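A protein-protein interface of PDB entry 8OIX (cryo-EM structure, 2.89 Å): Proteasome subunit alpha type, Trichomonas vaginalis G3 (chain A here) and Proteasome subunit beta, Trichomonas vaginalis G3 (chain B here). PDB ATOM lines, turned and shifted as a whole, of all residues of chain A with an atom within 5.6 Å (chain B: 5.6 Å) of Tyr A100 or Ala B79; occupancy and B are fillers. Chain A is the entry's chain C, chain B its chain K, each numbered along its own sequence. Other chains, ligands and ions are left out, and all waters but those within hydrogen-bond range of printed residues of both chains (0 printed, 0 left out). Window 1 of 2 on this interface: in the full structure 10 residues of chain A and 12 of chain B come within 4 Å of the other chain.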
ATOM      1  N   LYS A  95      -5.951  23.261  11.641  1.00  0.00           N
ATOM      2  CA  LYS A  95      -7.010  24.242  11.441  1.00  0.00           C
ATOM      3  C   LYS A  95      -6.607  25.268  10.392  1.00  0.00           C
ATOM      4  O   LYS A  95      -7.411  25.640   9.530  1.00  0.00           O
ATOM      5  CB  LYS A  95      -7.336  24.921  12.770  1.00  0.00           C
ATOM      6  CG  LYS A  95      -8.060  26.248  12.654  1.00  0.00           C
ATOM      7  CD  LYS A  95      -9.558  26.062  12.520  1.00  0.00           C
ATOM      8  CE  LYS A  95     -10.271  27.400  12.580  1.00  0.00           C
ATOM      9  NZ  LYS A  95      -9.973  28.120  13.848  1.00  0.00           N
ATOM     10  N   TYR A  96      -5.353  25.721  10.438  1.00  0.00           N
ATOM     11  CA  TYR A  96      -4.883  26.683   9.449  1.00  0.00           C
ATOM     12  C   TYR A  96      -4.790  26.044   8.072  1.00  0.00           C
ATOM     13  O   TYR A  96      -5.063  26.701   7.064  1.00  0.00           O
ATOM     14  CB  TYR A  96      -3.520  27.244   9.858  1.00  0.00           C
ATOM     15  CG  TYR A  96      -3.000  28.335   8.948  1.00  0.00           C
ATOM     16  CD1 TYR A  96      -2.342  28.031   7.763  1.00  0.00           C
ATOM     17  CD2 TYR A  96      -3.136  29.671   9.290  1.00  0.00           C
ATOM     18  CE1 TYR A  96      -1.865  29.022   6.935  1.00  0.00           C
ATOM     19  CE2 TYR A  96      -2.657  30.671   8.469  1.00  0.00           C
ATOM     20  CZ  TYR A  96      -2.022  30.340   7.293  1.00  0.00           C
ATOM     21  OH  TYR A  96      -1.541  31.333   6.472  1.00  0.00           O
ATOM     22  N   LEU A  97      -4.418  24.765   8.015  1.00  0.00           N
ATOM     23  CA  LEU A  97      -4.398  24.055   6.742  1.00  0.00           C
ATOM     24  C   LEU A  97      -5.805  23.898   6.182  1.00  0.00           C
ATOM     25  O   LEU A  97      -6.021  24.051   4.977  1.00  0.00           O
ATOM     26  CB  LEU A  97      -3.723  22.695   6.915  1.00  0.00           C
ATOM     27  CG  LEU A  97      -3.671  21.768   5.701  1.00  0.00           C
ATOM     28  CD1 LEU A  97      -3.057  22.476   4.509  1.00  0.00           C
ATOM     29  CD2 LEU A  97      -2.885  20.516   6.040  1.00  0.00           C
ATOM     30  N   LYS A  98      -6.775  23.583   7.040  1.00  0.00           N
ATOM     31  CA  LYS A  98      -8.155  23.467   6.586  1.00  0.00           C
ATOM     32  C   LYS A  98      -8.678  24.807   6.088  1.00  0.00           C
ATOM     33  O   LYS A  98      -9.388  24.870   5.078  1.00  0.00           O
ATOM     34  CB  LYS A  98      -9.032  22.936   7.720  1.00  0.00           C
ATOM     35  CG  LYS A  98     -10.271  22.194   7.255  1.00  0.00           C
ATOM     36  CD  LYS A  98     -11.358  22.208   8.314  1.00  0.00           C
ATOM     37  CE  LYS A  98     -10.854  21.657   9.632  1.00  0.00           C
ATOM     38  NZ  LYS A  98     -11.890  21.737  10.698  1.00  0.00           N
ATOM     39  N   THR A  99      -8.336  25.891   6.787  1.00  0.00           N
ATOM     40  CA  THR A  99      -8.859  27.204   6.424  1.00  0.00           C
ATOM     41  C   THR A  99      -8.206  27.751   5.159  1.00  0.00           C
ATOM     42  O   THR A  99      -8.890  28.324   4.305  1.00  0.00           O
ATOM     43  CB  THR A  99      -8.665  28.181   7.584  1.00  0.00           C
ATOM     44  OG1 THR A  99      -9.256  27.638   8.770  1.00  0.00           O
ATOM     45  CG2 THR A  99      -9.318  29.515   7.270  1.00  0.00           C
ATOM     46  N   TYR A 100      -6.891  27.588   5.012  1.00  0.00           N
ATOM     47  CA  TYR A 100      -6.156  28.218   3.922  1.00  0.00           C
ATOM     48  C   TYR A 100      -5.554  27.241   2.921  1.00  0.00           C
ATOM     49  O   TYR A 100      -4.917  27.688   1.962  1.00  0.00           O
ATOM     50  CB  TYR A 100      -5.043  29.105   4.491  1.00  0.00           C
ATOM     51  CG  TYR A 100      -5.522  30.138   5.486  1.00  0.00           C
ATOM     52  CD1 TYR A 100      -5.964  31.383   5.064  1.00  0.00           C
ATOM     53  CD2 TYR A 100      -5.537  29.865   6.845  1.00  0.00           C
ATOM     54  CE1 TYR A 100      -6.403  32.329   5.969  1.00  0.00           C
ATOM     55  CE2 TYR A 100      -5.976  30.806   7.757  1.00  0.00           C
ATOM     56  CZ  TYR A 100      -6.406  32.035   7.313  1.00  0.00           C
ATOM     57  OH  TYR A 100      -6.843  32.973   8.219  1.00  0.00           O
ATOM     58  N   ASP A 101      -5.739  25.931   3.105  1.00  0.00           N
ATOM     59  CA  ASP A 101      -5.118  24.912   2.248  1.00  0.00           C
ATOM     60  C   ASP A 101      -3.610  25.130   2.135  1.00  0.00           C
ATOM     61  O   ASP A 101      -2.982  24.774   1.135  1.00  0.00           O
ATOM     62  CB  ASP A 101      -5.774  24.877   0.865  1.00  0.00           C
ATOM     63  CG  ASP A 101      -5.383  23.653   0.058  1.00  0.00           C
ATOM     64  OD1 ASP A 101      -5.723  22.528   0.478  1.00  0.00           O
ATOM     65  OD2 ASP A 101      -4.735  23.818  -0.997  1.00  0.00           O
ATOM     66  N   GLU A 102      -3.021  25.722   3.168  1.00  0.00           N
ATOM     67  CA  GLU A 102      -1.596  25.999   3.210  1.00  0.00           C
ATOM     68  C   GLU A 102      -1.050  25.569   4.561  1.00  0.00           C
ATOM     69  O   GLU A 102      -1.747  25.635   5.577  1.00  0.00           O
ATOM     70  CB  GLU A 102      -1.320  27.496   2.960  1.00  0.00           C
ATOM     71  CG  GLU A 102       0.033  27.993   3.440  1.00  0.00           C
ATOM     72  CD  GLU A 102       0.287  29.444   3.089  1.00  0.00           C
ATOM     73  OE1 GLU A 102      -0.664  30.128   2.660  1.00  0.00           O
ATOM     74  OE2 GLU A 102       1.438  29.902   3.245  1.00  0.00           O
ATOM     75  N   TYR B  67      -4.946  39.483   8.896  1.00  0.00           N
ATOM     76  CA  TYR B  67      -3.894  38.490   8.705  1.00  0.00           C
ATOM     77  C   TYR B  67      -2.572  39.169   8.373  1.00  0.00           C
ATOM     78  O   TYR B  67      -1.509  38.737   8.831  1.00  0.00           O
ATOM     79  CB  TYR B  67      -4.295  37.509   7.602  1.00  0.00           C
ATOM     80  CG  TYR B  67      -3.260  36.449   7.297  1.00  0.00           C
ATOM     81  CD1 TYR B  67      -2.231  36.686   6.396  1.00  0.00           C
ATOM     82  CD2 TYR B  67      -3.324  35.202   7.902  1.00  0.00           C
ATOM     83  CE1 TYR B  67      -1.290  35.718   6.117  1.00  0.00           C
ATOM     84  CE2 TYR B  67      -2.387  34.227   7.627  1.00  0.00           C
ATOM     85  CZ  TYR B  67      -1.373  34.491   6.735  1.00  0.00           C
ATOM     86  OH  TYR B  67      -0.438  33.523   6.457  1.00  0.00           O
ATOM     87  N   LEU B  75      -1.577  37.175   2.751  1.00  0.00           N
ATOM     88  CA  LEU B  75      -2.146  35.928   2.263  1.00  0.00           C
ATOM     89  C   LEU B  75      -1.814  35.724   0.790  1.00  0.00           C
ATOM     90  O   LEU B  75      -1.743  36.674   0.008  1.00  0.00           O
ATOM     91  CB  LEU B  75      -3.664  35.916   2.446  1.00  0.00           C
ATOM     92  CG  LEU B  75      -4.236  35.528   3.806  1.00  0.00           C
ATOM     93  CD1 LEU B  75      -5.745  35.697   3.811  1.00  0.00           C
ATOM     94  CD2 LEU B  75      -3.854  34.102   4.146  1.00  0.00           C
ATOM     95  N   SER B  76      -1.607  34.465   0.416  1.00  0.00           N
ATOM     96  CA  SER B  76      -1.408  34.131  -0.983  1.00  0.00           C
ATOM     97  C   SER B  76      -2.746  34.217  -1.713  1.00  0.00           C
ATOM     98  O   SER B  76      -3.777  34.571  -1.136  1.00  0.00           O
ATOM     99  CB  SER B  76      -0.792  32.741  -1.115  1.00  0.00           C
ATOM    100  OG  SER B  76      -0.463  32.451  -2.461  1.00  0.00           O
ATOM    101  N   SER B  77      -2.745  33.883  -3.002  1.00  0.00           N
ATOM    102  CA  SER B  77      -4.020  33.809  -3.701  1.00  0.00           C
ATOM    103  C   SER B  77      -4.705  32.475  -3.458  1.00  0.00           C
ATOM    104  O   SER B  77      -5.934  32.427  -3.367  1.00  0.00           O
ATOM    105  CB  SER B  77      -3.831  34.041  -5.199  1.00  0.00           C
ATOM    106  OG  SER B  77      -3.414  35.369  -5.456  1.00  0.00           O
ATOM    107  N   ASP B  78      -3.933  31.398  -3.312  1.00  0.00           N
ATOM    108  CA  ASP B  78      -4.524  30.125  -2.921  1.00  0.00           C
ATOM    109  C   ASP B  78      -4.985  30.166  -1.472  1.00  0.00           C
ATOM    110  O   ASP B  78      -6.076  29.682  -1.147  1.00  0.00           O
ATOM    111  CB  ASP B  78      -3.524  28.991  -3.135  1.00  0.00           C
ATOM    112  CG  ASP B  78      -3.335  28.649  -4.597  1.00  0.00           C
ATOM    113  OD1 ASP B  78      -4.278  28.866  -5.385  1.00  0.00           O
ATOM    114  OD2 ASP B  78      -2.244  28.161  -4.958  1.00  0.00           O
ATOM    115  N   ALA B  79      -4.170  30.747  -0.588  1.00  0.00           N
ATOM    116  CA  ALA B  79      -4.556  30.845   0.815  1.00  0.00           C
ATOM    117  C   ALA B  79      -5.786  31.724   0.988  1.00  0.00           C
ATOM    118  O   ALA B  79      -6.713  31.365   1.720  1.00  0.00           O
ATOM    119  CB  ALA B  79      -3.391  31.381   1.644  1.00  0.00           C
ATOM    120  N   LEU B  80      -5.816  32.880   0.320  1.00  0.00           N
ATOM    121  CA  LEU B  80      -7.000  33.729   0.390  1.00  0.00           C
ATOM    122  C   LEU B  80      -8.205  33.046  -0.242  1.00  0.00           C
ATOM    123  O   LEU B  80      -9.319  33.139   0.281  1.00  0.00           O
ATOM    124  CB  LEU B  80      -6.738  35.080  -0.276  1.00  0.00           C
ATOM    125  CG  LEU B  80      -7.960  35.992  -0.402  1.00  0.00           C
ATOM    126  CD1 LEU B  80      -8.664  36.150   0.933  1.00  0.00           C
ATOM    127  CD2 LEU B  80      -7.552  37.343  -0.929  1.00  0.00           C
ATOM    128  N   ALA B  81      -8.007  32.368  -1.373  1.00  0.00           N
ATOM    129  CA  ALA B  81      -9.121  31.690  -2.023  1.00  0.00           C
ATOM    130  C   ALA B  81      -9.724  30.639  -1.107  1.00  0.00           C
ATOM    131  O   ALA B  81     -10.948  30.534  -0.986  1.00  0.00           O
ATOM    132  CB  ALA B  81      -8.660  31.060  -3.334  1.00  0.00           C
ATOM    133  N   HIS B  82      -8.878  29.868  -0.425  1.00  0.00           N
ATOM    134  CA  HIS B  82      -9.397  28.848   0.471  1.00  0.00           C
ATOM    135  C   HIS B  82      -9.953  29.447   1.756  1.00  0.00           C
ATOM    136  O   HIS B  82     -10.853  28.863   2.359  1.00  0.00           O
ATOM    137  CB  HIS B  82      -8.316  27.816   0.767  1.00  0.00           C
ATOM    138  CG  HIS B  82      -8.114  26.835  -0.345  1.00  0.00           C
ATOM    139  ND1 HIS B  82      -7.187  27.025  -1.346  1.00  0.00           N
ATOM    140  CD2 HIS B  82      -8.733  25.664  -0.623  1.00  0.00           C
ATOM    141  CE1 HIS B  82      -7.237  26.009  -2.188  1.00  0.00           C
ATOM    142  NE2 HIS B  82      -8.167  25.169  -1.772  1.00  0.00           N
ATOM    143  N   PHE B  83      -9.454  30.608   2.186  1.00  0.00           N
ATOM    144  CA  PHE B  83     -10.089  31.294   3.307  1.00  0.00           C
ATOM    145  C   PHE B  83     -11.496  31.756   2.944  1.00  0.00           C
ATOM    146  O   PHE B  83     -12.432  31.607   3.740  1.00  0.00           O
ATOM    147  CB  PHE B  83      -9.237  32.477   3.759  1.00  0.00           C
ATOM    148  CG  PHE B  83      -9.915  33.351   4.768  1.00  0.00           C
ATOM    149  CD1 PHE B  83     -10.063  32.926   6.077  1.00  0.00           C
ATOM    150  CD2 PHE B  83     -10.411  34.592   4.410  1.00  0.00           C
ATOM    151  CE1 PHE B  83     -10.690  33.723   7.009  1.00  0.00           C
ATOM    152  CE2 PHE B  83     -11.039  35.392   5.340  1.00  0.00           C
ATOM    153  CZ  PHE B  83     -11.180  34.955   6.641  1.00  0.00           C
ATOM    154  N   ILE B  84     -11.661  32.320   1.747  1.00  0.00           N
ATOM    155  CA  ILE B  84     -12.992  32.682   1.269  1.00  0.00           C
ATOM    156  C   ILE B  84     -13.866  31.442   1.171  1.00  0.00           C
ATOM    157  O   ILE B  84     -15.052  31.470   1.516  1.00  0.00           O
ATOM    158  CB  ILE B  84     -12.908  33.417  -0.083  1.00  0.00           C
ATOM    159  CG1 ILE B  84     -11.933  34.593  -0.004  1.00  0.00           C
ATOM    160  CG2 ILE B  84     -14.293  33.879  -0.521  1.00  0.00           C
ATOM    161  CD1 ILE B  84     -12.289  35.757  -0.898  1.00  0.00           C
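Of chain B, only Leu B75 (3.6 Å), Asp B78 (3.9 Å), Ala B79 (3.4 Å), His B82 (3.5 Å) and Phe B83 (3.6 Å) come within 4 Å of Tyr A100. Of chain A, only Tyr A100 and Glu A102 come within 4 Å of Ala B79. Printed residues of chain A within 4 Å of Phe B83: Thr A99 and Tyr A100. Of the printed residues of chain B, Thr A99 touches His B82 (2.8 Å) and Phe B83 (3.2 Å). Lys A98 touches none of the printed residues of chain B. The nearest printed residue of chain B that does not touch Tyr A96 is Leu B75 (4.3 Å).
Among the printed residues, no Asp or Glu carboxylate lies within 4 Å of a Lys or Arg side-chain nitrogen of the other chain.
The backbone carbonyl oxygen of Asp B78 sits at hydrogen-bond distance from a ring nitrogen (ND1) of His B82 (2.9 Å). The backbone carbonyl oxygen (O) of Lys A95 lies within hydrogen-bond range of the side-chain hydroxyl (OG1) of Thr A99 (2.8 Å).
Among the printed residues, pairs that only touch across the chains: Tyr A100 with Leu B75, Tyr A100 with Asp B78, Tyr A100 with Ala B79, Tyr A100 with His B82, Tyr A100 with Phe B83, Asp A101 with His B82 and Glu A102 with Ala B79.
The side-chain hydroxyl (OH) of Tyr A96 sits at hydrogen-bond distance from the side-chain hydroxyl (OH) of Tyr B67 (2.5 Å). The backbone NH of Phe B83 is in hydrogen-bond range of the backbone carbonyl oxygen of Thr A99 (3.2 Å). The backbone carbonyl oxygen (O) of Thr A99 sits close to the backbone carbonyl oxygen (O) of His B82 (2.8 Å).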
